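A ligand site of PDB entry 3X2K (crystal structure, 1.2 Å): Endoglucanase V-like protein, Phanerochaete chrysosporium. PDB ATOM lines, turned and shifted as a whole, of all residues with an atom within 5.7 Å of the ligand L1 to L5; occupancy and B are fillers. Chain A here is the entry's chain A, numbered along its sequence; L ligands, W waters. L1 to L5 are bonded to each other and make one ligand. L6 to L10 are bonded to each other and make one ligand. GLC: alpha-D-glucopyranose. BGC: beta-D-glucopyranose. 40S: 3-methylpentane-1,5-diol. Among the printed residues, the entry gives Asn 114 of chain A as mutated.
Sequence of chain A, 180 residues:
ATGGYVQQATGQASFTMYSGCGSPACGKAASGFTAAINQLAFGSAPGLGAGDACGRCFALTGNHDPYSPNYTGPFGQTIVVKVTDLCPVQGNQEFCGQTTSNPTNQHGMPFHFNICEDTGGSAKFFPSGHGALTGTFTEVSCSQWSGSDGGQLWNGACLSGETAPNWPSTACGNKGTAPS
The backbone carbonyl oxygen of Asn 155 is in hydrogen-bond range of an oxygen (O2) of BGC L5 (2.6 Å). The backbone carbonyl oxygen (O) of Pro 24 is in hydrogen-bond range of an oxygen (O6) of BGC L3 (3.4 Å). O of Leu 153 sits at hydrogen-bond distance from O08 of 40S L11 (2.8 Å). NE1 of Trp 154 lies within hydrogen-bond range of O6 of BGC L3, at 2.9 Å. N of Gly 47 is in hydrogen-bond range of O2 of BGC L3. An oxygen (O3) of BGC L3 sits at hydrogen-bond distance from the backbone NH (N) of Leu 48. O6 of GLC L1 sits at hydrogen-bond distance from ND2 of Asn 114 (2.9 Å). N of Gly 49 is in hydrogen-bond range of O3 of BGC L3, 3.0 Å away. The side-chain amide oxygen of Asn 92 is in hydrogen-bond range of an oxygen (O6) of BGC L10 (2.7 Å). O4 of BGC L10 is in hydrogen-bond range of ND2 of Asn 114. The backbone carbonyl oxygen (O) of Gly 47 is in hydrogen-bond range of an oxygen (O6) of BGC L4. O2 of BGC L2 lies within hydrogen-bond range of OD2 of Asp 85 (2.8 Å). An oxygen (O2) of GLC L1 sits at hydrogen-bond distance from the side-chain amide nitrogen of Asn 92. The backbone carbonyl oxygen of Ser 23 is in hydrogen-bond range of an oxygen (O3) of BGC L2.
O1 of GLC L1 is in hydrogen-bond range of O4 of BGC L10 (2.6 Å).
OD2 of Asp 85 sits at hydrogen-bond distance from OH of Tyr 18 (2.6 Å). SG of Cys 87 sits at hydrogen-bond distance from ND2 of Asn 114 (3.7 Å). O of Gln 90 is in hydrogen-bond range of ND2 of Asn 92 (2.9 Å). The backbone NH of Ala 36 sits at hydrogen-bond distance from the backbone carbonyl oxygen of Asn 114, 2.8 Å away. OD1 of Asp 85 sits at hydrogen-bond distance from N of Ala 25 (2.9 Å).
Residues that only touch the ligand L1 to L5: Tyr 18 (3.3 Å), Gly 20 (3.5 Å), Ala 25 (3.3 Å), Ala 36 (3.2 Å), Ala 45 (3.9 Å), Pro 46 (3.5 Å), Leu 86 (3.3 Å) and Pro 88 (3.7 Å). Of the 25 residues printed, 18 come within 4 Å of the ligand L1 to L5.
Water W10 lies within hydrogen-bond range of O2 of GLC L1, NE2 of Gln 90 and ND2 of Asn 92. Water W5 lies within hydrogen-bond range of O2 of BGC L3 (2.7 Å), O of Gly 49 (2.8 Å) and O of Ala 45 (2.8 Å). Water W15 bridges an oxygen (O2) of BGC L4 (2.8 Å) and an oxygen (O05) of 40S L12 (2.9 Å). Water W9 lies within hydrogen-bond range of O of Gly 20 (2.8 Å) and O2 of BGC L2 (2.9 Å). Water W12 lies within hydrogen-bond range of the backbone carbonyl oxygen of Gly 20 (2.9 Å), an oxygen (O2) of BGC L2 (3.0 Å) and the backbone NH of Ser 23 (3.1 Å).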
ATOM      1  N   TYR A  18     -16.956 -13.233   1.878  1.00  0.00           N
ATOM      2  CA  TYR A  18     -16.588 -11.963   1.258  1.00  0.00           C
ATOM      3  C   TYR A  18     -15.107 -11.777   1.346  1.00  0.00           C
ATOM      4  O   TYR A  18     -14.424 -12.468   2.108  1.00  0.00           O
ATOM      5  CB  TYR A  18     -17.309 -10.781   1.903  1.00  0.00           C
ATOM      6  CG  TYR A  18     -16.723 -10.240   3.196  1.00  0.00           C
ATOM      7  CD1 TYR A  18     -16.836 -10.958   4.396  1.00  0.00           C
ATOM      8  CD2 TYR A  18     -16.106  -8.980   3.242  1.00  0.00           C
ATOM      9  CE1 TYR A  18     -16.356 -10.435   5.589  1.00  0.00           C
ATOM     10  CE2 TYR A  18     -15.639  -8.463   4.434  1.00  0.00           C
ATOM     11  CZ  TYR A  18     -15.767  -9.195   5.612  1.00  0.00           C
ATOM     12  OH  TYR A  18     -15.309  -8.697   6.822  1.00  0.00           O
ATOM     13  N   GLY A  20     -11.737  -8.830   1.447  1.00  0.00           N
ATOM     14  CA  GLY A  20     -11.318  -7.470   1.747  1.00  0.00           C
ATOM     15  C   GLY A  20     -11.740  -6.997   3.127  1.00  0.00           C
ATOM     16  O   GLY A  20     -12.587  -6.109   3.276  1.00  0.00           O
ATOM     17  N   CYS A  21     -11.166  -7.602   4.160  1.00  0.00           N
ATOM     18  CA  CYS A  21     -11.500  -7.239   5.528  1.00  0.00           C
ATOM     19  C   CYS A  21     -10.297  -6.681   6.275  1.00  0.00           C
ATOM     20  O   CYS A  21     -10.214  -6.767   7.498  1.00  0.00           O
ATOM     21  CB  CYS A  21     -12.119  -8.405   6.276  1.00  0.00           C
ATOM     22  SG  CYS A  21     -11.113  -9.912   6.308  1.00  0.00           S
ATOM     23  N   SER A  23      -9.523  -3.446   6.490  1.00  0.00           N
ATOM     24  CA  SER A  23      -9.846  -2.185   7.152  1.00  0.00           C
ATOM     25  C   SER A  23     -11.281  -2.231   7.641  1.00  0.00           C
ATOM     26  O   SER A  23     -12.134  -1.425   7.247  1.00  0.00           O
ATOM     27  CB  SER A  23      -9.608  -1.011   6.218  1.00  0.00           C
ATOM     28  OG  SER A  23     -10.322  -1.150   5.006  1.00  0.00           O
ATOM     29  N   PRO A  24     -11.579  -3.185   8.531  1.00  0.00           N
ATOM     30  CA  PRO A  24     -12.957  -3.505   8.863  1.00  0.00           C
ATOM     31  C   PRO A  24     -13.571  -2.520   9.848  1.00  0.00           C
ATOM     32  O   PRO A  24     -12.901  -1.659  10.428  1.00  0.00           O
ATOM     33  CB  PRO A  24     -12.836  -4.904   9.488  1.00  0.00           C
ATOM     34  CG  PRO A  24     -11.535  -4.804  10.231  1.00  0.00           C
ATOM     35  CD  PRO A  24     -10.621  -3.995   9.307  1.00  0.00           C
ATOM     36  N   ALA A  25     -14.879  -2.668  10.037  1.00  0.00           N
ATOM     37  CA  ALA A  25     -15.651  -1.675  10.776  1.00  0.00           C
ATOM     38  C   ALA A  25     -15.306  -1.563  12.245  1.00  0.00           C
ATOM     39  O   ALA A  25     -15.551  -0.524  12.852  1.00  0.00           O
ATOM     40  CB  ALA A  25     -17.150  -1.925  10.606  1.00  0.00           C
ATOM     41  N   GLY A  27     -12.264  -1.475  13.290  1.00  0.00           N
ATOM     42  CA  GLY A  27     -11.071  -0.668  13.336  1.00  0.00           C
ATOM     43  C   GLY A  27      -9.791  -1.424  13.650  1.00  0.00           C
ATOM     44  O   GLY A  27      -8.718  -0.828  13.733  1.00  0.00           O
ATOM     45  N   ALA A  36     -17.735 -10.663   9.236  1.00  0.00           N
ATOM     46  CA  ALA A  36     -18.643  -9.560   9.441  1.00  0.00           C
ATOM     47  C   ALA A  36     -19.974 -10.163   9.916  1.00  0.00           C
ATOM     48  O   ALA A  36     -20.359 -11.252   9.491  1.00  0.00           O
ATOM     49  CB  ALA A  36     -18.871  -8.800   8.140  1.00  0.00           C
ATOM     50  N   ALA A  45     -23.356   1.425  12.185  1.00  0.00           N
ATOM     51  CA  ALA A  45     -23.776   1.661  10.812  1.00  0.00           C
ATOM     52  C   ALA A  45     -22.539   2.068  10.025  1.00  0.00           C
ATOM     53  O   ALA A  45     -21.547   2.499  10.642  1.00  0.00           O
ATOM     54  CB  ALA A  45     -24.842   2.764  10.731  1.00  0.00           C
ATOM     55  N   PRO A  46     -22.571   1.956   8.686  1.00  0.00           N
ATOM     56  CA  PRO A  46     -21.420   2.386   7.881  1.00  0.00           C
ATOM     57  C   PRO A  46     -20.947   3.774   8.296  1.00  0.00           C
ATOM     58  O   PRO A  46     -21.757   4.714   8.378  1.00  0.00           O
ATOM     59  CB  PRO A  46     -21.967   2.374   6.455  1.00  0.00           C
ATOM     60  CG  PRO A  46     -22.986   1.236   6.493  1.00  0.00           C
ATOM     61  CD  PRO A  46     -23.637   1.370   7.840  1.00  0.00           C
ATOM     62  N   GLY A  47     -19.646   3.895   8.538  1.00  0.00           N
ATOM     63  CA  GLY A  47     -19.026   5.152   8.905  1.00  0.00           C
ATOM     64  C   GLY A  47     -18.911   5.451  10.394  1.00  0.00           C
ATOM     65  O   GLY A  47     -18.125   6.318  10.784  1.00  0.00           O
ATOM     66  N   LEU A  48     -19.694   4.756  11.221  1.00  0.00           N
ATOM     67  CA  LEU A  48     -19.748   5.080  12.654  1.00  0.00           C
ATOM     68  C   LEU A  48     -18.757   4.286  13.503  1.00  0.00           C
ATOM     69  O   LEU A  48     -18.693   4.477  14.716  1.00  0.00           O
ATOM     70  CB  LEU A  48     -21.162   4.905  13.195  1.00  0.00           C
ATOM     71  CG  LEU A  48     -22.272   5.666  12.455  1.00  0.00           C
ATOM     72  CD1 LEU A  48     -23.589   5.486  13.206  1.00  0.00           C
ATOM     73  CD2 LEU A  48     -21.908   7.134  12.268  1.00  0.00           C
ATOM     74  N   GLY A  49     -18.001   3.390  12.884  1.00  0.00           N
ATOM     75  CA  GLY A  49     -17.008   2.633  13.623  1.00  0.00           C
ATOM     76  C   GLY A  49     -17.558   1.419  14.368  1.00  0.00           C
ATOM     77  O   GLY A  49     -18.558   0.821  13.940  1.00  0.00           O
ATOM     78  N   ASP A  85     -16.091  -7.026  11.643  1.00  0.00           N
ATOM     79  CA  ASP A  85     -16.631  -6.217  10.544  1.00  0.00           C
ATOM     80  C   ASP A  85     -18.162  -6.245  10.513  1.00  0.00           C
ATOM     81  O   ASP A  85     -18.812  -7.073  11.190  1.00  0.00           O
ATOM     82  CB  ASP A  85     -16.013  -6.726   9.222  1.00  0.00           C
ATOM     83  CG  ASP A  85     -15.972  -5.682   8.108  1.00  0.00           C
ATOM     84  OD1 ASP A  85     -16.345  -4.502   8.353  1.00  0.00           O
ATOM     85  OD2 ASP A  85     -15.551  -6.069   6.989  1.00  0.00           O
ATOM     86  N   LEU A  86     -18.702  -5.309   9.726  1.00  0.00           N
ATOM     87  CA  LEU A  86     -20.139  -5.038   9.615  1.00  0.00           C
ATOM     88  C   LEU A  86     -20.610  -5.394   8.223  1.00  0.00           C
ATOM     89  O   LEU A  86     -20.079  -4.851   7.242  1.00  0.00           O
ATOM     90  CB  LEU A  86     -20.338  -3.529   9.868  1.00  0.00           C
ATOM     91  CG  LEU A  86     -21.750  -2.937  10.053  1.00  0.00           C
ATOM     92  CD1 LEU A  86     -21.639  -1.454  10.345  1.00  0.00           C
ATOM     93  CD2 LEU A  86     -22.657  -3.119   8.884  1.00  0.00           C
ATOM     94  N   CYS A  87     -21.612  -6.275   8.125  1.00  0.00           N
ATOM     95  CA  CYS A  87     -22.247  -6.583   6.859  1.00  0.00           C
ATOM     96  C   CYS A  87     -23.487  -5.702   6.770  1.00  0.00           C
ATOM     97  O   CYS A  87     -24.460  -5.951   7.482  1.00  0.00           O
ATOM     98  CB  CYS A  87     -22.601  -8.063   6.745  1.00  0.00           C
ATOM     99  SG  CYS A  87     -23.283  -8.487   5.123  1.00  0.00           S
ATOM    100  N   PRO A  88     -23.441  -4.630   5.959  1.00  0.00           N
ATOM    101  CA  PRO A  88     -24.504  -3.631   5.998  1.00  0.00           C
ATOM    102  C   PRO A  88     -25.790  -4.084   5.313  1.00  0.00           C
ATOM    103  O   PRO A  88     -25.778  -4.932   4.415  1.00  0.00           O
ATOM    104  CB  PRO A  88     -23.886  -2.474   5.209  1.00  0.00           C
ATOM    105  CG  PRO A  88     -23.037  -3.183   4.158  1.00  0.00           C
ATOM    106  CD  PRO A  88     -22.425  -4.320   4.930  1.00  0.00           C
ATOM    107  N   GLN A  90     -27.431  -2.072   3.408  1.00  0.00           N
ATOM    108  CA  GLN A  90     -27.312  -1.502   2.077  1.00  0.00           C
ATOM    109  C   GLN A  90     -26.588  -2.469   1.153  1.00  0.00           C
ATOM    110  O   GLN A  90     -25.512  -2.950   1.470  1.00  0.00           O
ATOM    111  CB  GLN A  90     -26.562  -0.154   2.126  1.00  0.00           C
ATOM    112  CG  GLN A  90     -26.532   0.570   0.788  1.00  0.00           C
ATOM    113  CD  GLN A  90     -25.489   0.039  -0.194  1.00  0.00           C
ATOM    114  OE1 GLN A  90     -25.777  -0.139  -1.387  1.00  0.00           O
ATOM    115  NE2 GLN A  90     -24.278  -0.201   0.288  1.00  0.00           N
ATOM    116  N   GLY A  91     -27.204  -2.756   0.000  1.00  0.00           N
ATOM    117  CA  GLY A  91     -26.592  -3.566  -1.034  1.00  0.00           C
ATOM    118  C   GLY A  91     -26.506  -5.045  -0.735  1.00  0.00           C
ATOM    119  O   GLY A  91     -25.986  -5.795  -1.556  1.00  0.00           O
ATOM    120  N   ASN A  92     -26.992  -5.462   0.422  1.00  0.00           N
ATOM    121  CA  ASN A  92     -26.827  -6.839   0.890  1.00  0.00           C
ATOM    122  C   ASN A  92     -28.078  -7.301   1.585  1.00  0.00           C
ATOM    123  O   ASN A  92     -28.042  -7.952   2.618  1.00  0.00           O
ATOM    124  CB  ASN A  92     -25.612  -6.940   1.825  1.00  0.00           C
ATOM    125  CG  ASN A  92     -24.309  -6.627   1.104  1.00  0.00           C
ATOM    126  OD1 ASN A  92     -23.626  -7.520   0.599  1.00  0.00           O
ATOM    127  ND2 ASN A  92     -23.964  -5.340   1.044  1.00  0.00           N
ATOM    128  N   ASN A 114     -20.880 -13.152   7.452  1.00  0.00           N
ATOM    129  CA  ASN A 114     -20.172 -13.043   6.182  1.00  0.00           C
ATOM    130  C   ASN A 114     -18.707 -13.357   6.526  1.00  0.00           C
ATOM    131  O   ASN A 114     -18.021 -12.548   7.168  1.00  0.00           O
ATOM    132  CB  ASN A 114     -20.330 -11.603   5.675  1.00  0.00           C
ATOM    133  CG  ASN A 114     -20.260 -11.468   4.166  1.00  0.00           C
ATOM    134  OD1 ASN A 114     -20.160 -12.466   3.436  1.00  0.00           O
ATOM    135  ND2 ASN A 114     -20.315 -10.221   3.698  1.00  0.00           N
ATOM    136  N   LEU A 153      -6.642   1.051  13.275  1.00  0.00           N
ATOM    137  CA  LEU A 153      -6.661   1.811  12.043  1.00  0.00           C
ATOM    138  C   LEU A 153      -7.037   3.274  12.260  1.00  0.00           C
ATOM    139  O   LEU A 153      -6.736   4.138  11.430  1.00  0.00           O
ATOM    140  CB  LEU A 153      -7.657   1.181  11.073  1.00  0.00           C
ATOM    141  CG  LEU A 153      -7.166  -0.150  10.517  1.00  0.00           C
ATOM    142  CD1 LEU A 153      -8.316  -1.071  10.213  1.00  0.00           C
ATOM    143  CD2 LEU A 153      -6.339   0.072   9.279  1.00  0.00           C
ATOM    144  N   TRP A 154      -7.709   3.545  13.374  1.00  0.00           N
ATOM    145  CA  TRP A 154      -8.229   4.878  13.657  1.00  0.00           C
ATOM    146  C   TRP A 154      -8.599   4.906  15.139  1.00  0.00           C
ATOM    147  O   TRP A 154      -8.749   3.862  15.781  1.00  0.00           O
ATOM    148  CB  TRP A 154      -9.409   5.265  12.757  1.00  0.00           C
ATOM    149  CG  TRP A 154     -10.291   4.129  12.236  1.00  0.00           C
ATOM    150  CD1 TRP A 154     -10.209   3.516  11.004  1.00  0.00           C
ATOM    151  CD2 TRP A 154     -11.353   3.464  12.927  1.00  0.00           C
ATOM    152  NE1 TRP A 154     -11.161   2.540  10.899  1.00  0.00           N
ATOM    153  CE2 TRP A 154     -11.891   2.488  12.057  1.00  0.00           C
ATOM    154  CE3 TRP A 154     -11.943   3.621  14.189  1.00  0.00           C
ATOM    155  CZ2 TRP A 154     -12.986   1.689  12.402  1.00  0.00           C
ATOM    156  CZ3 TRP A 154     -13.016   2.824  14.536  1.00  0.00           C
ATOM    157  CH2 TRP A 154     -13.517   1.856  13.649  1.00  0.00           C
ATOM    158  N   ASN A 155      -8.700   6.106  15.691  1.00  0.00           N
ATOM    159  CA  ASN A 155      -9.008   6.220  17.109  1.00  0.00           C
ATOM    160  C   ASN A 155     -10.389   5.643  17.410  1.00  0.00           C
ATOM    161  O   ASN A 155     -11.324   5.831  16.631  1.00  0.00           O
ATOM    162  CB  ASN A 155      -8.993   7.680  17.533  1.00  0.00           C
ATOM    163  CG  ASN A 155      -7.628   8.341  17.412  1.00  0.00           C
ATOM    164  OD1 ASN A 155      -6.589   7.694  17.403  1.00  0.00           O
ATOM    165  ND2 ASN A 155      -7.643   9.664  17.320  1.00  0.00           N
ATOM    166  N   GLY A 156     -10.522   4.937  18.527  1.00  0.00           N
ATOM    167  CA  GLY A 156     -11.794   4.348  18.888  1.00  0.00           C
ATOM    168  C   GLY A 156     -11.995   2.957  18.317  1.00  0.00           C
ATOM    169  O   GLY A 156     -13.052   2.363  18.547  1.00  0.00           O
HETATM  170  C1  GLC L   1     -20.617  -6.425   1.788  1.00  0.00           C
HETATM  171  C2  GLC L   1     -20.671  -4.922   1.603  1.00  0.00           C
HETATM  172  C3  GLC L   1     -19.357  -4.265   2.040  1.00  0.00           C
HETATM  173  C4  GLC L   1     -18.964  -4.759   3.409  1.00  0.00           C
HETATM  174  C5  GLC L   1     -18.960  -6.258   3.449  1.00  0.00           C
HETATM  175  C6  GLC L   1     -18.662  -6.729   4.899  1.00  0.00           C
HETATM  176  O1  GLC L   1     -19.763  -7.021   0.818  1.00  0.00           O
HETATM  177  O2  GLC L   1     -21.011  -4.580   0.288  1.00  0.00           O
HETATM  178  O3  GLC L   1     -19.516  -2.856   2.005  1.00  0.00           O
HETATM  179  O4  GLC L   1     -17.627  -4.254   3.636  1.00  0.00           O
HETATM  180  O5  GLC L   1     -20.217  -6.726   3.098  1.00  0.00           O
HETATM  181  O6  GLC L   1     -18.879  -8.135   5.040  1.00  0.00           O
HETATM  182  C2  BGC L   2     -16.019  -3.158   4.917  1.00  0.00           C
HETATM  183  C3  BGC L   2     -15.745  -2.231   6.104  1.00  0.00           C
HETATM  184  C4  BGC L   2     -16.852  -1.222   6.310  1.00  0.00           C
HETATM  185  C5  BGC L   2     -18.204  -1.935   6.290  1.00  0.00           C
HETATM  186  C6  BGC L   2     -19.376  -1.035   6.620  1.00  0.00           C
HETATM  187  C1  BGC L   2     -17.469  -3.628   4.900  1.00  0.00           C
HETATM  188  O2  BGC L   2     -15.151  -4.286   4.919  1.00  0.00           O
HETATM  189  O3  BGC L   2     -14.498  -1.603   5.832  1.00  0.00           O
HETATM  190  O4  BGC L   2     -16.721  -0.630   7.602  1.00  0.00           O
HETATM  191  O5  BGC L   2     -18.343  -2.545   5.008  1.00  0.00           O
HETATM  192  O6  BGC L   2     -19.440   0.032   5.688  1.00  0.00           O
HETATM  193  C2  BGC L   3     -16.842   1.354   8.860  1.00  0.00           C
HETATM  194  C3  BGC L   3     -16.305   2.805   8.959  1.00  0.00           C
HETATM  195  C4  BGC L   3     -14.807   2.822   8.837  1.00  0.00           C
HETATM  196  C5  BGC L   3     -14.373   2.014   7.626  1.00  0.00           C
HETATM  197  C6  BGC L   3     -12.854   1.871   7.524  1.00  0.00           C
HETATM  198  C1  BGC L   3     -16.320   0.729   7.608  1.00  0.00           C
HETATM  199  O2  BGC L   3     -18.258   1.376   8.839  1.00  0.00           O
HETATM  200  O3  BGC L   3     -16.731   3.362  10.169  1.00  0.00           O
HETATM  201  O4  BGC L   3     -14.376   4.178   8.615  1.00  0.00           O
HETATM  202  O5  BGC L   3     -14.909   0.706   7.678  1.00  0.00           O
HETATM  203  O6  BGC L   3     -12.340   1.166   8.662  1.00  0.00           O
HETATM  204  C2  BGC L   4     -12.902   5.948   9.205  1.00  0.00           C
HETATM  205  C3  BGC L   4     -12.251   6.630  10.395  1.00  0.00           C
HETATM  206  C4  BGC L   4     -13.242   6.963  11.481  1.00  0.00           C
HETATM  207  C5  BGC L   4     -14.099   5.749  11.795  1.00  0.00           C
HETATM  208  C6  BGC L   4     -15.191   6.029  12.801  1.00  0.00           C
HETATM  209  C1  BGC L   4     -13.709   4.771   9.715  1.00  0.00           C
HETATM  210  O2  BGC L   4     -11.898   5.527   8.301  1.00  0.00           O
HETATM  211  O3  BGC L   4     -11.552   7.794   9.945  1.00  0.00           O
HETATM  212  O4  BGC L   4     -12.496   7.262  12.687  1.00  0.00           O
HETATM  213  O5  BGC L   4     -14.684   5.204  10.592  1.00  0.00           O
HETATM  214  O6  BGC L   4     -16.048   7.086  12.367  1.00  0.00           O
HETATM  215  C2  BGC L   5     -12.185   8.471  14.722  1.00  0.00           C
HETATM  216  C3  BGC L   5     -12.197   9.835  15.373  1.00  0.00           C
HETATM  217  C4  BGC L   5     -11.579  10.848  14.433  1.00  0.00           C
HETATM  218  C5  BGC L   5     -12.354  10.780  13.136  1.00  0.00           C
HETATM  219  C6  BGC L   5     -11.835  11.793  12.096  1.00  0.00           C
HETATM  220  C1  BGC L   5     -12.815   8.478  13.338  1.00  0.00           C
HETATM  221  O2  BGC L   5     -12.901   7.535  15.523  1.00  0.00           O
HETATM  222  O3  BGC L   5     -11.455   9.833  16.607  1.00  0.00           O
HETATM  223  O4  BGC L   5     -11.610  12.139  14.982  1.00  0.00           O
HETATM  224  O5  BGC L   5     -12.223   9.462  12.566  1.00  0.00           O
HETATM  225  O6  BGC L   5     -10.438  11.563  11.882  1.00  0.00           O
HETATM  226  C2  BGC L   6     -27.943 -30.007  -8.252  1.00  0.00           C
HETATM  227  C3  BGC L   6     -28.251 -28.597  -7.708  1.00  0.00           C
HETATM  228  C4  BGC L   6     -27.825 -27.538  -8.706  1.00  0.00           C
HETATM  229  C5  BGC L   6     -28.527 -27.815 -10.068  1.00  0.00           C
HETATM  230  C6  BGC L   6     -28.089 -26.831 -11.176  1.00  0.00           C
HETATM  231  C1  BGC L   6     -28.602 -30.204  -9.610  1.00  0.00           C
HETATM  232  O1  BGC L   6     -28.041 -31.413 -10.169  1.00  0.00           O
HETATM  233  O2  BGC L   6     -28.407 -30.993  -7.347  1.00  0.00           O
HETATM  234  O3  BGC L   6     -27.575 -28.434  -6.449  1.00  0.00           O
HETATM  235  O4  BGC L   6     -28.263 -26.264  -8.286  1.00  0.00           O
HETATM  236  O5  BGC L   6     -28.219 -29.135 -10.461  1.00  0.00           O
HETATM  237  O6  BGC L   6     -26.674 -26.768 -11.135  1.00  0.00           O
HETATM  238  C2  BGC L   7     -27.722 -23.973  -8.220  1.00  0.00           C
HETATM  239  C3  BGC L   7     -26.602 -22.965  -7.918  1.00  0.00           C
HETATM  240  C4  BGC L   7     -26.168 -23.232  -6.474  1.00  0.00           C
HETATM  241  C5  BGC L   7     -25.721 -24.697  -6.292  1.00  0.00           C
HETATM  242  C6  BGC L   7     -25.418 -25.019  -4.840  1.00  0.00           C
HETATM  243  C1  BGC L   7     -27.175 -25.389  -8.089  1.00  0.00           C
HETATM  244  O2  BGC L   7     -28.360 -23.702  -9.422  1.00  0.00           O
HETATM  245  O3  BGC L   7     -27.116 -21.677  -8.138  1.00  0.00           O
HETATM  246  O4  BGC L   7     -25.022 -22.415  -6.222  1.00  0.00           O
HETATM  247  O5  BGC L   7     -26.760 -25.590  -6.746  1.00  0.00           O
HETATM  248  O6  BGC L   7     -26.606 -24.744  -4.095  1.00  0.00           O
HETATM  249  C2  BGC L   8     -23.804 -21.034  -4.754  1.00  0.00           C
HETATM  250  C3  BGC L   8     -23.942 -19.882  -3.754  1.00  0.00           C
HETATM  251  C4  BGC L   8     -24.657 -18.710  -4.415  1.00  0.00           C
HETATM  252  C5  BGC L   8     -25.978 -19.161  -5.062  1.00  0.00           C
HETATM  253  C6  BGC L   8     -26.679 -18.073  -5.903  1.00  0.00           C
HETATM  254  C1  BGC L   8     -25.194 -21.387  -5.277  1.00  0.00           C
HETATM  255  O2  BGC L   8     -23.168 -22.163  -4.090  1.00  0.00           O
HETATM  256  O3  BGC L   8     -22.632 -19.517  -3.249  1.00  0.00           O
HETATM  257  O4  BGC L   8     -25.017 -17.761  -3.417  1.00  0.00           O
HETATM  258  O5  BGC L   8     -25.698 -20.278  -5.928  1.00  0.00           O
HETATM  259  O6  BGC L   8     -25.784 -17.692  -6.963  1.00  0.00           O
HETATM  260  C2  BGC L   9     -25.013 -15.547  -2.648  1.00  0.00           C
HETATM  261  C3  BGC L   9     -24.181 -14.273  -2.643  1.00  0.00           C
HETATM  262  C4  BGC L   9     -22.767 -14.563  -2.113  1.00  0.00           C
HETATM  263  C5  BGC L   9     -22.131 -15.820  -2.755  1.00  0.00           C
HETATM  264  C6  BGC L   9     -20.816 -16.155  -2.034  1.00  0.00           C
HETATM  265  C1  BGC L   9     -24.243 -16.626  -3.388  1.00  0.00           C
HETATM  266  O2  BGC L   9     -26.249 -15.214  -3.283  1.00  0.00           O
HETATM  267  O3  BGC L   9     -24.788 -13.274  -1.798  1.00  0.00           O
HETATM  268  O4  BGC L   9     -21.922 -13.432  -2.408  1.00  0.00           O
HETATM  269  O5  BGC L   9     -23.041 -16.886  -2.646  1.00  0.00           O
HETATM  270  O6  BGC L   9     -20.976 -16.401  -0.624  1.00  0.00           O
HETATM  271  C2  BGC L  10     -20.418 -11.793  -1.776  1.00  0.00           C
HETATM  272  C3  BGC L  10     -20.019 -10.793  -0.698  1.00  0.00           C
HETATM  273  C4  BGC L  10     -21.241 -10.188  -0.043  1.00  0.00           C
HETATM  274  C5  BGC L  10     -22.125 -11.345   0.460  1.00  0.00           C
HETATM  275  C6  BGC L  10     -23.348 -10.929   1.243  1.00  0.00           C
HETATM  276  C1  BGC L  10     -21.422 -12.786  -1.263  1.00  0.00           C
HETATM  277  O2  BGC L  10     -19.203 -12.484  -2.130  1.00  0.00           O
HETATM  278  O3  BGC L  10     -19.247  -9.717  -1.272  1.00  0.00           O
HETATM  279  O4  BGC L  10     -20.796  -9.399   1.038  1.00  0.00           O
HETATM  280  O5  BGC L  10     -22.513 -12.112  -0.676  1.00  0.00           O
HETATM  281  O6  BGC L  10     -24.206 -10.115   0.457  1.00  0.00           O
HETATM  282  C01 40S L  11      -9.574   3.113   7.073  1.00  0.00           C
HETATM  283  C02 40S L  11      -8.165   2.978   6.539  1.00  0.00           C
HETATM  284  C03 40S L  11      -8.283   2.495   5.099  1.00  0.00           C
HETATM  285  C04 40S L  11      -7.090   1.722   4.621  1.00  0.00           C
HETATM  286  O05 40S L  11      -7.290   1.245   3.294  1.00  0.00           O
HETATM  287  C06 40S L  11      -7.379   4.276   6.681  1.00  0.00           C
HETATM  288  C07 40S L  11      -7.147   4.746   8.112  1.00  0.00           C
HETATM  289  O08 40S L  11      -6.185   3.887   8.737  1.00  0.00           O
HETATM  290  C01 40S L  12     -16.469   9.912   6.131  1.00  0.00           C
HETATM  291  C02 40S L  12     -16.187   8.455   6.388  1.00  0.00           C
HETATM  292  C03 40S L  12     -14.737   8.086   6.168  1.00  0.00           C
HETATM  293  C04 40S L  12     -14.342   8.123   4.699  1.00  0.00           C
HETATM  294  O05 40S L  12     -13.060   7.546   4.582  1.00  0.00           O
HETATM  295  C06 40S L  12     -16.647   8.049   7.779  1.00  0.00           C
HETATM  296  C07 40S L  12     -18.102   8.431   7.999  1.00  0.00           C
HETATM  297  O08 40S L  12     -18.888   7.761   7.038  1.00  0.00           O
HETATM  298  O   HOH W   1     -15.521   7.629  16.618  1.00  0.00           O
HETATM  299  O   HOH W   2      -9.815   7.105   7.269  1.00  0.00           O
HETATM  300  O   HOH W   3     -20.343  -0.592   3.230  1.00  0.00           O
HETATM  301  O   HOH W   4     -19.309  -1.615  -0.448  1.00  0.00           O
HETATM  302  O   HOH W   5     -19.338   0.868  11.277  1.00  0.00           O
HETATM  303  O   HOH W   6     -19.466  -5.059  -1.962  1.00  0.00           O
HETATM  304  O   HOH W   7     -18.407   2.562   5.419  1.00  0.00           O
HETATM  305  O   HOH W   8     -14.213   0.570   4.005  1.00  0.00           O
HETATM  306  O   HOH W   9     -15.215  -5.600   2.313  1.00  0.00           O
HETATM  307  O   HOH W  10     -22.648  -2.616  -0.070  1.00  0.00           O
HETATM  308  O   HOH W  11      -9.756  13.318  16.296  1.00  0.00           O
HETATM  309  O   HOH W  12     -12.187  -3.815   5.036  1.00  0.00           O
HETATM  310  O   HOH W  13      -9.435   8.933  11.525  1.00  0.00           O
HETATM  311  O   HOH W  14     -17.077   8.629  14.432  1.00  0.00           O
HETATM  312  O   HOH W  15     -12.910   4.894   5.813  1.00  0.00           O
HETATM  313  O   HOH W  16     -17.055  -6.600   0.439  1.00  0.00           O
